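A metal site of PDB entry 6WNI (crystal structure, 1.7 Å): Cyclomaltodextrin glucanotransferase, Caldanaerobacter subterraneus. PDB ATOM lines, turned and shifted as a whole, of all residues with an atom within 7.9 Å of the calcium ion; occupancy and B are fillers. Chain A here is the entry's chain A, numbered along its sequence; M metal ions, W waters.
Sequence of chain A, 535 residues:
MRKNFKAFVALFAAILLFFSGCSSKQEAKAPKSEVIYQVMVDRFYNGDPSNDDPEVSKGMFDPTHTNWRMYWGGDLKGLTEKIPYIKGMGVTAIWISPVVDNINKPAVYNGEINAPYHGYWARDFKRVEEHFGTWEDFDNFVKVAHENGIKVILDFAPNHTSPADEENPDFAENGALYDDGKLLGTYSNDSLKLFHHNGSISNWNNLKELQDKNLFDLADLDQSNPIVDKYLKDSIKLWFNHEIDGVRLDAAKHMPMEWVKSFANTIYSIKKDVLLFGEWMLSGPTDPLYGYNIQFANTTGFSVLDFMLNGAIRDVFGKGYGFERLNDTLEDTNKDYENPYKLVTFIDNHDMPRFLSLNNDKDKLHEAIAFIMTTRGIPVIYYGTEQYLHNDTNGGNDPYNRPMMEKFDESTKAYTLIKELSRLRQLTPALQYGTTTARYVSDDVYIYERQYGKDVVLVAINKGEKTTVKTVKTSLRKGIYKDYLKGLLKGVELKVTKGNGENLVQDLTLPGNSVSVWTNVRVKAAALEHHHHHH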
ATOM      1  N   PRO A 158      33.086  -6.505 -23.816  1.00  0.00           N
ATOM      2  CA  PRO A 158      31.697  -6.838 -23.446  1.00  0.00           C
ATOM      3  C   PRO A 158      30.795  -5.638 -23.233  1.00  0.00           C
ATOM      4  O   PRO A 158      29.670  -5.805 -22.766  1.00  0.00           O
ATOM      5  CB  PRO A 158      31.891  -7.609 -22.123  1.00  0.00           C
ATOM      6  CG  PRO A 158      33.069  -6.934 -21.482  1.00  0.00           C
ATOM      7  CD  PRO A 158      33.991  -6.557 -22.652  1.00  0.00           C
ATOM      8  N   ASN A 159      31.243  -4.417 -23.571  1.00  0.00           N
ATOM      9  CA  ASN A 159      30.368  -3.251 -23.435  1.00  0.00           C
ATOM     10  C   ASN A 159      29.283  -3.218 -24.499  1.00  0.00           C
ATOM     11  O   ASN A 159      28.214  -2.636 -24.283  1.00  0.00           O
ATOM     12  CB  ASN A 159      31.195  -1.966 -23.494  1.00  0.00           C
ATOM     13  CG  ASN A 159      30.320  -0.711 -23.420  1.00  0.00           C
ATOM     14  OD1 ASN A 159      29.743  -0.403 -22.374  1.00  0.00           O
ATOM     15  ND2 ASN A 159      30.252   0.027 -24.510  1.00  0.00           N
ATOM     16  N   HIS A 160      29.540  -3.816 -25.662  1.00  0.00           N
ATOM     17  CA  HIS A 160      28.723  -3.492 -26.826  1.00  0.00           C
ATOM     18  C   HIS A 160      28.915  -4.585 -27.863  1.00  0.00           C
ATOM     19  O   HIS A 160      29.832  -5.396 -27.787  1.00  0.00           O
ATOM     20  CB  HIS A 160      29.103  -2.148 -27.437  1.00  0.00           C
ATOM     21  CG  HIS A 160      30.551  -2.027 -27.778  1.00  0.00           C
ATOM     22  ND1 HIS A 160      31.438  -1.281 -27.022  1.00  0.00           N
ATOM     23  CD2 HIS A 160      31.289  -2.586 -28.766  1.00  0.00           C
ATOM     24  CE1 HIS A 160      32.648  -1.366 -27.549  1.00  0.00           C
ATOM     25  NE2 HIS A 160      32.589  -2.158 -28.605  1.00  0.00           N
ATOM     26  N   HIS A 196      20.763  -1.396 -24.020  1.00  0.00           N
ATOM     27  CA  HIS A 196      20.247  -0.098 -23.623  1.00  0.00           C
ATOM     28  C   HIS A 196      19.707   0.621 -24.850  1.00  0.00           C
ATOM     29  O   HIS A 196      20.339   0.624 -25.913  1.00  0.00           O
ATOM     30  CB  HIS A 196      21.327   0.769 -22.961  1.00  0.00           C
ATOM     31  CG  HIS A 196      21.750   0.280 -21.612  1.00  0.00           C
ATOM     32  ND1 HIS A 196      23.033  -0.122 -21.339  1.00  0.00           N
ATOM     33  CD2 HIS A 196      21.044   0.116 -20.466  1.00  0.00           C
ATOM     34  CE1 HIS A 196      23.114  -0.512 -20.076  1.00  0.00           C
ATOM     35  NE2 HIS A 196      21.919  -0.380 -19.534  1.00  0.00           N
ATOM     36  N   ILE A 201      26.074   8.545 -25.966  1.00  0.00           N
ATOM     37  CA  ILE A 201      26.724   9.370 -24.948  1.00  0.00           C
ATOM     38  C   ILE A 201      26.959  10.771 -25.486  1.00  0.00           C
ATOM     39  O   ILE A 201      27.479  10.944 -26.598  1.00  0.00           O
ATOM     40  CB  ILE A 201      28.038   8.725 -24.481  1.00  0.00           C
ATOM     41  CG1 ILE A 201      27.783   7.376 -23.819  1.00  0.00           C
ATOM     42  CG2 ILE A 201      28.759   9.666 -23.495  1.00  0.00           C
ATOM     43  CD1 ILE A 201      29.045   6.569 -23.579  1.00  0.00           C
ATOM     44  N   LYS A 208      26.950   8.027 -15.289  1.00  0.00           N
ATOM     45  CA  LYS A 208      25.725   7.242 -15.621  1.00  0.00           C
ATOM     46  C   LYS A 208      25.541   7.232 -17.139  1.00  0.00           C
ATOM     47  O   LYS A 208      25.175   6.205 -17.668  1.00  0.00           O
ATOM     48  CB  LYS A 208      24.477   7.847 -14.959  1.00  0.00           C
ATOM     49  CG  LYS A 208      23.926   7.067 -13.786  1.00  0.00           C
ATOM     50  CD  LYS A 208      23.886   5.584 -13.946  1.00  0.00           C
ATOM     51  CE  LYS A 208      23.188   4.898 -12.795  1.00  0.00           C
ATOM     52  NZ  LYS A 208      23.804   3.617 -12.408  1.00  0.00           N
ATOM     53  N   GLU A 209      25.737   8.386 -17.787  1.00  0.00           N
ATOM     54  CA  GLU A 209      25.646   8.453 -19.238  1.00  0.00           C
ATOM     55  C   GLU A 209      26.690   7.565 -19.891  1.00  0.00           C
ATOM     56  O   GLU A 209      26.382   6.834 -20.848  1.00  0.00           O
ATOM     57  CB  GLU A 209      25.804   9.916 -19.668  1.00  0.00           C
ATOM     58  CG  GLU A 209      25.770  10.142 -21.153  1.00  0.00           C
ATOM     59  CD  GLU A 209      24.904  11.312 -21.538  1.00  0.00           C
ATOM     60  OE1 GLU A 209      25.162  11.934 -22.592  1.00  0.00           O
ATOM     61  OE2 GLU A 209      23.967  11.618 -20.773  1.00  0.00           O
ATOM     62  N   LEU A 210      27.933   7.607 -19.398  1.00  0.00           N
ATOM     63  CA  LEU A 210      28.983   6.768 -19.965  1.00  0.00           C
ATOM     64  C   LEU A 210      28.645   5.290 -19.872  1.00  0.00           C
ATOM     65  O   LEU A 210      29.041   4.506 -20.744  1.00  0.00           O
ATOM     66  CB  LEU A 210      30.314   7.049 -19.271  1.00  0.00           C
ATOM     67  CG  LEU A 210      30.923   8.425 -19.511  1.00  0.00           C
ATOM     68  CD1 LEU A 210      32.051   8.628 -18.527  1.00  0.00           C
ATOM     69  CD2 LEU A 210      31.414   8.602 -20.931  1.00  0.00           C
ATOM     70  N   GLN A 211      27.936   4.871 -18.822  1.00  0.00           N
ATOM     71  CA  GLN A 211      27.623   3.449 -18.638  1.00  0.00           C
ATOM     72  C   GLN A 211      26.358   3.015 -19.369  1.00  0.00           C
ATOM     73  O   GLN A 211      26.308   1.906 -19.908  1.00  0.00           O
ATOM     74  CB  GLN A 211      27.481   3.126 -17.155  1.00  0.00           C
ATOM     75  CG  GLN A 211      28.726   3.367 -16.319  1.00  0.00           C
ATOM     76  CD  GLN A 211      28.505   3.039 -14.861  1.00  0.00           C
ATOM     77  OE1 GLN A 211      27.372   2.761 -14.444  1.00  0.00           O
ATOM     78  NE2 GLN A 211      29.576   3.082 -14.073  1.00  0.00           N
ATOM     79  N   ASP A 212      25.350   3.874 -19.397  1.00  0.00           N
ATOM     80  CA  ASP A 212      24.006   3.484 -19.796  1.00  0.00           C
ATOM     81  C   ASP A 212      23.632   3.885 -21.221  1.00  0.00           C
ATOM     82  O   ASP A 212      22.589   3.448 -21.717  1.00  0.00           O
ATOM     83  CB  ASP A 212      22.980   4.077 -18.827  1.00  0.00           C
ATOM     84  CG  ASP A 212      22.966   3.356 -17.496  1.00  0.00           C
ATOM     85  OD1 ASP A 212      23.748   2.407 -17.320  1.00  0.00           O
ATOM     86  OD2 ASP A 212      22.149   3.746 -16.627  1.00  0.00           O
ATOM     87  N   LYS A 213      24.435   4.709 -21.881  1.00  0.00           N
ATOM     88  CA  LYS A 213      24.176   5.106 -23.256  1.00  0.00           C
ATOM     89  C   LYS A 213      25.199   4.451 -24.189  1.00  0.00           C
ATOM     90  O   LYS A 213      26.136   3.787 -23.737  1.00  0.00           O
ATOM     91  CB  LYS A 213      24.193   6.624 -23.414  1.00  0.00           C
ATOM     92  CG  LYS A 213      22.989   7.311 -22.766  1.00  0.00           C
ATOM     93  CD  LYS A 213      22.919   8.770 -23.173  1.00  0.00           C
ATOM     94  CE  LYS A 213      21.730   9.480 -22.537  1.00  0.00           C
ATOM     95  NZ  LYS A 213      21.690  10.894 -22.982  1.00  0.00           N
ATOM     96  N   ASN A 214      24.995   4.665 -25.486  1.00  0.00           N
ATOM     97  CA  ASN A 214      25.801   4.030 -26.523  1.00  0.00           C
ATOM     98  C   ASN A 214      27.090   4.804 -26.758  1.00  0.00           C
ATOM     99  O   ASN A 214      27.074   6.013 -26.989  1.00  0.00           O
ATOM    100  CB  ASN A 214      25.051   3.944 -27.853  1.00  0.00           C
ATOM    101  CG  ASN A 214      23.848   3.014 -27.810  1.00  0.00           C
ATOM    102  OD1 ASN A 214      23.695   2.195 -26.913  1.00  0.00           O
ATOM    103  ND2 ASN A 214      22.990   3.140 -28.801  1.00  0.00           N
ATOM    104  N   LEU A 215      28.211   4.091 -26.737  1.00  0.00           N
ATOM    105  CA  LEU A 215      29.480   4.624 -27.224  1.00  0.00           C
ATOM    106  C   LEU A 215      29.380   4.781 -28.738  1.00  0.00           C
ATOM    107  O   LEU A 215      29.453   3.794 -29.465  1.00  0.00           O
ATOM    108  CB  LEU A 215      30.610   3.682 -26.821  1.00  0.00           C
ATOM    109  CG  LEU A 215      32.029   4.044 -27.232  1.00  0.00           C
ATOM    110  CD1 LEU A 215      32.378   5.410 -26.682  1.00  0.00           C
ATOM    111  CD2 LEU A 215      32.993   2.982 -26.709  1.00  0.00           C
ATOM    112  N   LEU A 218      27.429   2.231 -31.163  1.00  0.00           N
ATOM    113  CA  LEU A 218      27.629   0.839 -30.748  1.00  0.00           C
ATOM    114  C   LEU A 218      26.526   0.415 -29.799  1.00  0.00           C
ATOM    115  O   LEU A 218      26.362   1.007 -28.726  1.00  0.00           O
ATOM    116  CB  LEU A 218      28.996   0.688 -30.085  1.00  0.00           C
ATOM    117  CG  LEU A 218      30.192   1.052 -30.961  1.00  0.00           C
ATOM    118  CD1 LEU A 218      31.473   0.974 -30.116  1.00  0.00           C
ATOM    119  CD2 LEU A 218      30.277   0.111 -32.177  1.00  0.00           C
ATOM    120  N   ALA A 219      25.767  -0.598 -30.193  1.00  0.00           N
ATOM    121  CA  ALA A 219      24.684  -1.138 -29.362  1.00  0.00           C
ATOM    122  C   ALA A 219      25.177  -1.530 -27.977  1.00  0.00           C
ATOM    123  O   ALA A 219      25.920  -2.490 -27.822  1.00  0.00           O
ATOM    124  CB  ALA A 219      24.039  -2.354 -30.050  1.00  0.00           C
ATOM    125  N   ASP A 220      24.746  -0.791 -26.965  1.00  0.00           N
ATOM    126  CA  ASP A 220      25.259  -0.999 -25.614  1.00  0.00           C
ATOM    127  C   ASP A 220      24.551  -2.173 -24.964  1.00  0.00           C
ATOM    128  O   ASP A 220      23.330  -2.155 -24.801  1.00  0.00           O
ATOM    129  CB  ASP A 220      25.057   0.266 -24.786  1.00  0.00           C
ATOM    130  CG  ASP A 220      26.037   0.359 -23.646  1.00  0.00           C
ATOM    131  OD1 ASP A 220      27.260   0.375 -23.937  1.00  0.00           O
ATOM    132  OD2 ASP A 220      25.599   0.398 -22.467  1.00  0.00           O
ATOM    133  N   LEU A 221      25.322  -3.187 -24.545  1.00  0.00           N
ATOM    134  CA  LEU A 221      24.764  -4.305 -23.814  1.00  0.00           C
ATOM    135  C   LEU A 221      24.407  -3.873 -22.386  1.00  0.00           C
ATOM    136  O   LEU A 221      25.056  -3.017 -21.789  1.00  0.00           O
ATOM    137  CB  LEU A 221      25.760  -5.466 -23.781  1.00  0.00           C
ATOM    138  CG  LEU A 221      26.029  -6.103 -25.150  1.00  0.00           C
ATOM    139  CD1 LEU A 221      27.256  -6.980 -25.101  1.00  0.00           C
ATOM    140  CD2 LEU A 221      24.801  -6.935 -25.578  1.00  0.00           C
ATOM    141  N   ASP A 222      23.337  -4.484 -21.875  1.00  0.00           N
ATOM    142  CA  ASP A 222      22.802  -4.185 -20.542  1.00  0.00           C
ATOM    143  C   ASP A 222      23.203  -5.343 -19.637  1.00  0.00           C
ATOM    144  O   ASP A 222      22.492  -6.355 -19.552  1.00  0.00           O
ATOM    145  CB  ASP A 222      21.278  -4.001 -20.607  1.00  0.00           C
ATOM    146  CG  ASP A 222      20.661  -3.632 -19.271  1.00  0.00           C
ATOM    147  OD1 ASP A 222      21.322  -3.786 -18.215  1.00  0.00           O
ATOM    148  OD2 ASP A 222      19.477  -3.200 -19.268  1.00  0.00           O
ATOM    149  N   GLN A 223      24.341  -5.207 -18.950  1.00  0.00           N
ATOM    150  CA  GLN A 223      24.790  -6.285 -18.090  1.00  0.00           C
ATOM    151  C   GLN A 223      23.884  -6.499 -16.876  1.00  0.00           C
ATOM    152  O   GLN A 223      24.019  -7.534 -16.215  1.00  0.00           O
ATOM    153  CB  GLN A 223      26.237  -6.047 -17.629  1.00  0.00           C
ATOM    154  CG  GLN A 223      27.263  -5.984 -18.756  1.00  0.00           C
ATOM    155  CD  GLN A 223      27.316  -4.625 -19.418  1.00  0.00           C
ATOM    156  OE1 GLN A 223      26.749  -3.654 -18.904  1.00  0.00           O
ATOM    157  NE2 GLN A 223      27.990  -4.542 -20.558  1.00  0.00           N
ATOM    158  N   ALA A 251      36.935  -0.626 -23.146  1.00  0.00           N
ATOM    159  CA  ALA A 251      35.883   0.324 -22.761  1.00  0.00           C
ATOM    160  C   ALA A 251      35.439   0.144 -21.304  1.00  0.00           C
ATOM    161  O   ALA A 251      34.249   0.162 -20.999  1.00  0.00           O
ATOM    162  CB  ALA A 251      34.695   0.225 -23.719  1.00  0.00           C
ATOM    163  N   LYS A 253      35.456   2.031 -18.735  1.00  0.00           N
ATOM    164  CA  LYS A 253      34.733   3.172 -18.100  1.00  0.00           C
ATOM    165  C   LYS A 253      33.247   3.168 -18.488  1.00  0.00           C
ATOM    166  O   LYS A 253      32.471   3.886 -17.885  1.00  0.00           O
ATOM    167  CB  LYS A 253      35.421   4.496 -18.444  1.00  0.00           C
ATOM    168  CG  LYS A 253      34.985   5.210 -19.696  1.00  0.00           C
ATOM    169  CD  LYS A 253      36.079   6.060 -20.290  1.00  0.00           C
ATOM    170  CE  LYS A 253      35.814   7.541 -20.359  1.00  0.00           C
ATOM    171  NZ  LYS A 253      37.026   8.287 -20.728  1.00  0.00           N
ATOM    172  N   HIS A 254      32.845   2.335 -19.456  1.00  0.00           N
ATOM    173  CA  HIS A 254      31.477   2.339 -19.958  1.00  0.00           C
ATOM    174  C   HIS A 254      30.615   1.224 -19.392  1.00  0.00           C
ATOM    175  O   HIS A 254      29.480   1.036 -19.851  1.00  0.00           O
ATOM    176  CB  HIS A 254      31.478   2.261 -21.483  1.00  0.00           C
ATOM    177  CG  HIS A 254      32.076   3.465 -22.123  1.00  0.00           C
ATOM    178  ND1 HIS A 254      31.419   4.676 -22.201  1.00  0.00           N
ATOM    179  CD2 HIS A 254      33.281   3.655 -22.707  1.00  0.00           C
ATOM    180  CE1 HIS A 254      32.192   5.553 -22.811  1.00  0.00           C
ATOM    181  NE2 HIS A 254      33.324   4.960 -23.124  1.00  0.00           N
ATOM    182  N   MET A 255      31.105   0.476 -18.422  1.00  0.00           N
ATOM    183  CA  MET A 255      30.316  -0.529 -17.753  1.00  0.00           C
ATOM    184  C   MET A 255      30.284  -0.262 -16.259  1.00  0.00           C
ATOM    185  O   MET A 255      31.213   0.360 -15.715  1.00  0.00           O
ATOM    186  CB  MET A 255      30.873  -1.926 -18.031  1.00  0.00           C
ATOM    187  CG  MET A 255      30.767  -2.288 -19.509  1.00  0.00           C
ATOM    188  SD  MET A 255      31.749  -3.724 -19.956  1.00  0.00           S
ATOM    189  CE  MET A 255      33.412  -3.032 -19.949  1.00  0.00           C
ATOM    190  N   PRO A 256      29.209  -0.661 -15.570  1.00  0.00           N
ATOM    191  CA  PRO A 256      29.150  -0.485 -14.114  1.00  0.00           C
ATOM    192  C   PRO A 256      30.345  -1.123 -13.435  1.00  0.00           C
ATOM    193  O   PRO A 256      30.625  -2.307 -13.623  1.00  0.00           O
ATOM    194  CB  PRO A 256      27.841  -1.184 -13.728  1.00  0.00           C
ATOM    195  CG  PRO A 256      27.002  -1.088 -14.964  1.00  0.00           C
ATOM    196  CD  PRO A 256      27.949  -1.184 -16.124  1.00  0.00           C
HETATM  197 CA    CA M   1      27.675   0.269 -21.228  1.00  0.00          CA
HETATM  198  O   HOH W   1      26.930  -1.020 -19.286  1.00  0.00           O
HETATM  199  O   HOH W   2      28.148   2.377 -22.278  1.00  0.00           O
HETATM  200  O   HOH W   3      27.366  -2.093 -21.959  1.00  0.00           O
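A ring nitrogen (ND1) of His 254 sits at hydrogen-bond distance from the backbone carbonyl oxygen of Leu 210, 2.8 Å away. The backbone NH (N) of His 196 lies within hydrogen-bond range of the backbone carbonyl oxygen (O) of Asp 220, at 2.8 Å. The backbone NH (N) of Asp 220 is in hydrogen-bond range of the side-chain amide oxygen (OD1) of Asn 214 (3.2 Å). N of Leu 221 lies within hydrogen-bond range of O of Asn 159, at 3.0 Å. The side-chain sulfur (SD) of Met 255 sits at hydrogen-bond distance from the backbone NH (N) of Asn 159 (3.7 Å). The side-chain amide nitrogen (ND2) of Asn 159 lies within hydrogen-bond range of a ring nitrogen (ND1) of His 160 (3.1 Å).
Of the 24 residues printed, 4 come within 4 Å of the calcium ion.
The calcium ion is bound by the backbone carbonyl oxygen (O) of His 254 (2.4 Å), water W2 (2.4 Å), the side-chain carboxylate (OD2) of Asp 220 (2.4 Å), water W1 (2.4 Å), the side-chain amide oxygen (OD1) of Asn 159 (2.5 Å), water W3 (2.5 Å), the backbone carbonyl oxygen (O) of Gln 211 (2.5 Å) and the side-chain carboxylate (OD1) of Asp 220 (2.7 Å).
Water W3 lies within hydrogen-bond range of the backbone carbonyl oxygen (O) of Leu 221 (2.5 Å), the backbone carbonyl oxygen (O) of Asn 159 (2.5 Å) and the side-chain amide nitrogen (NE2) of Gln 223 (2.9 Å).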
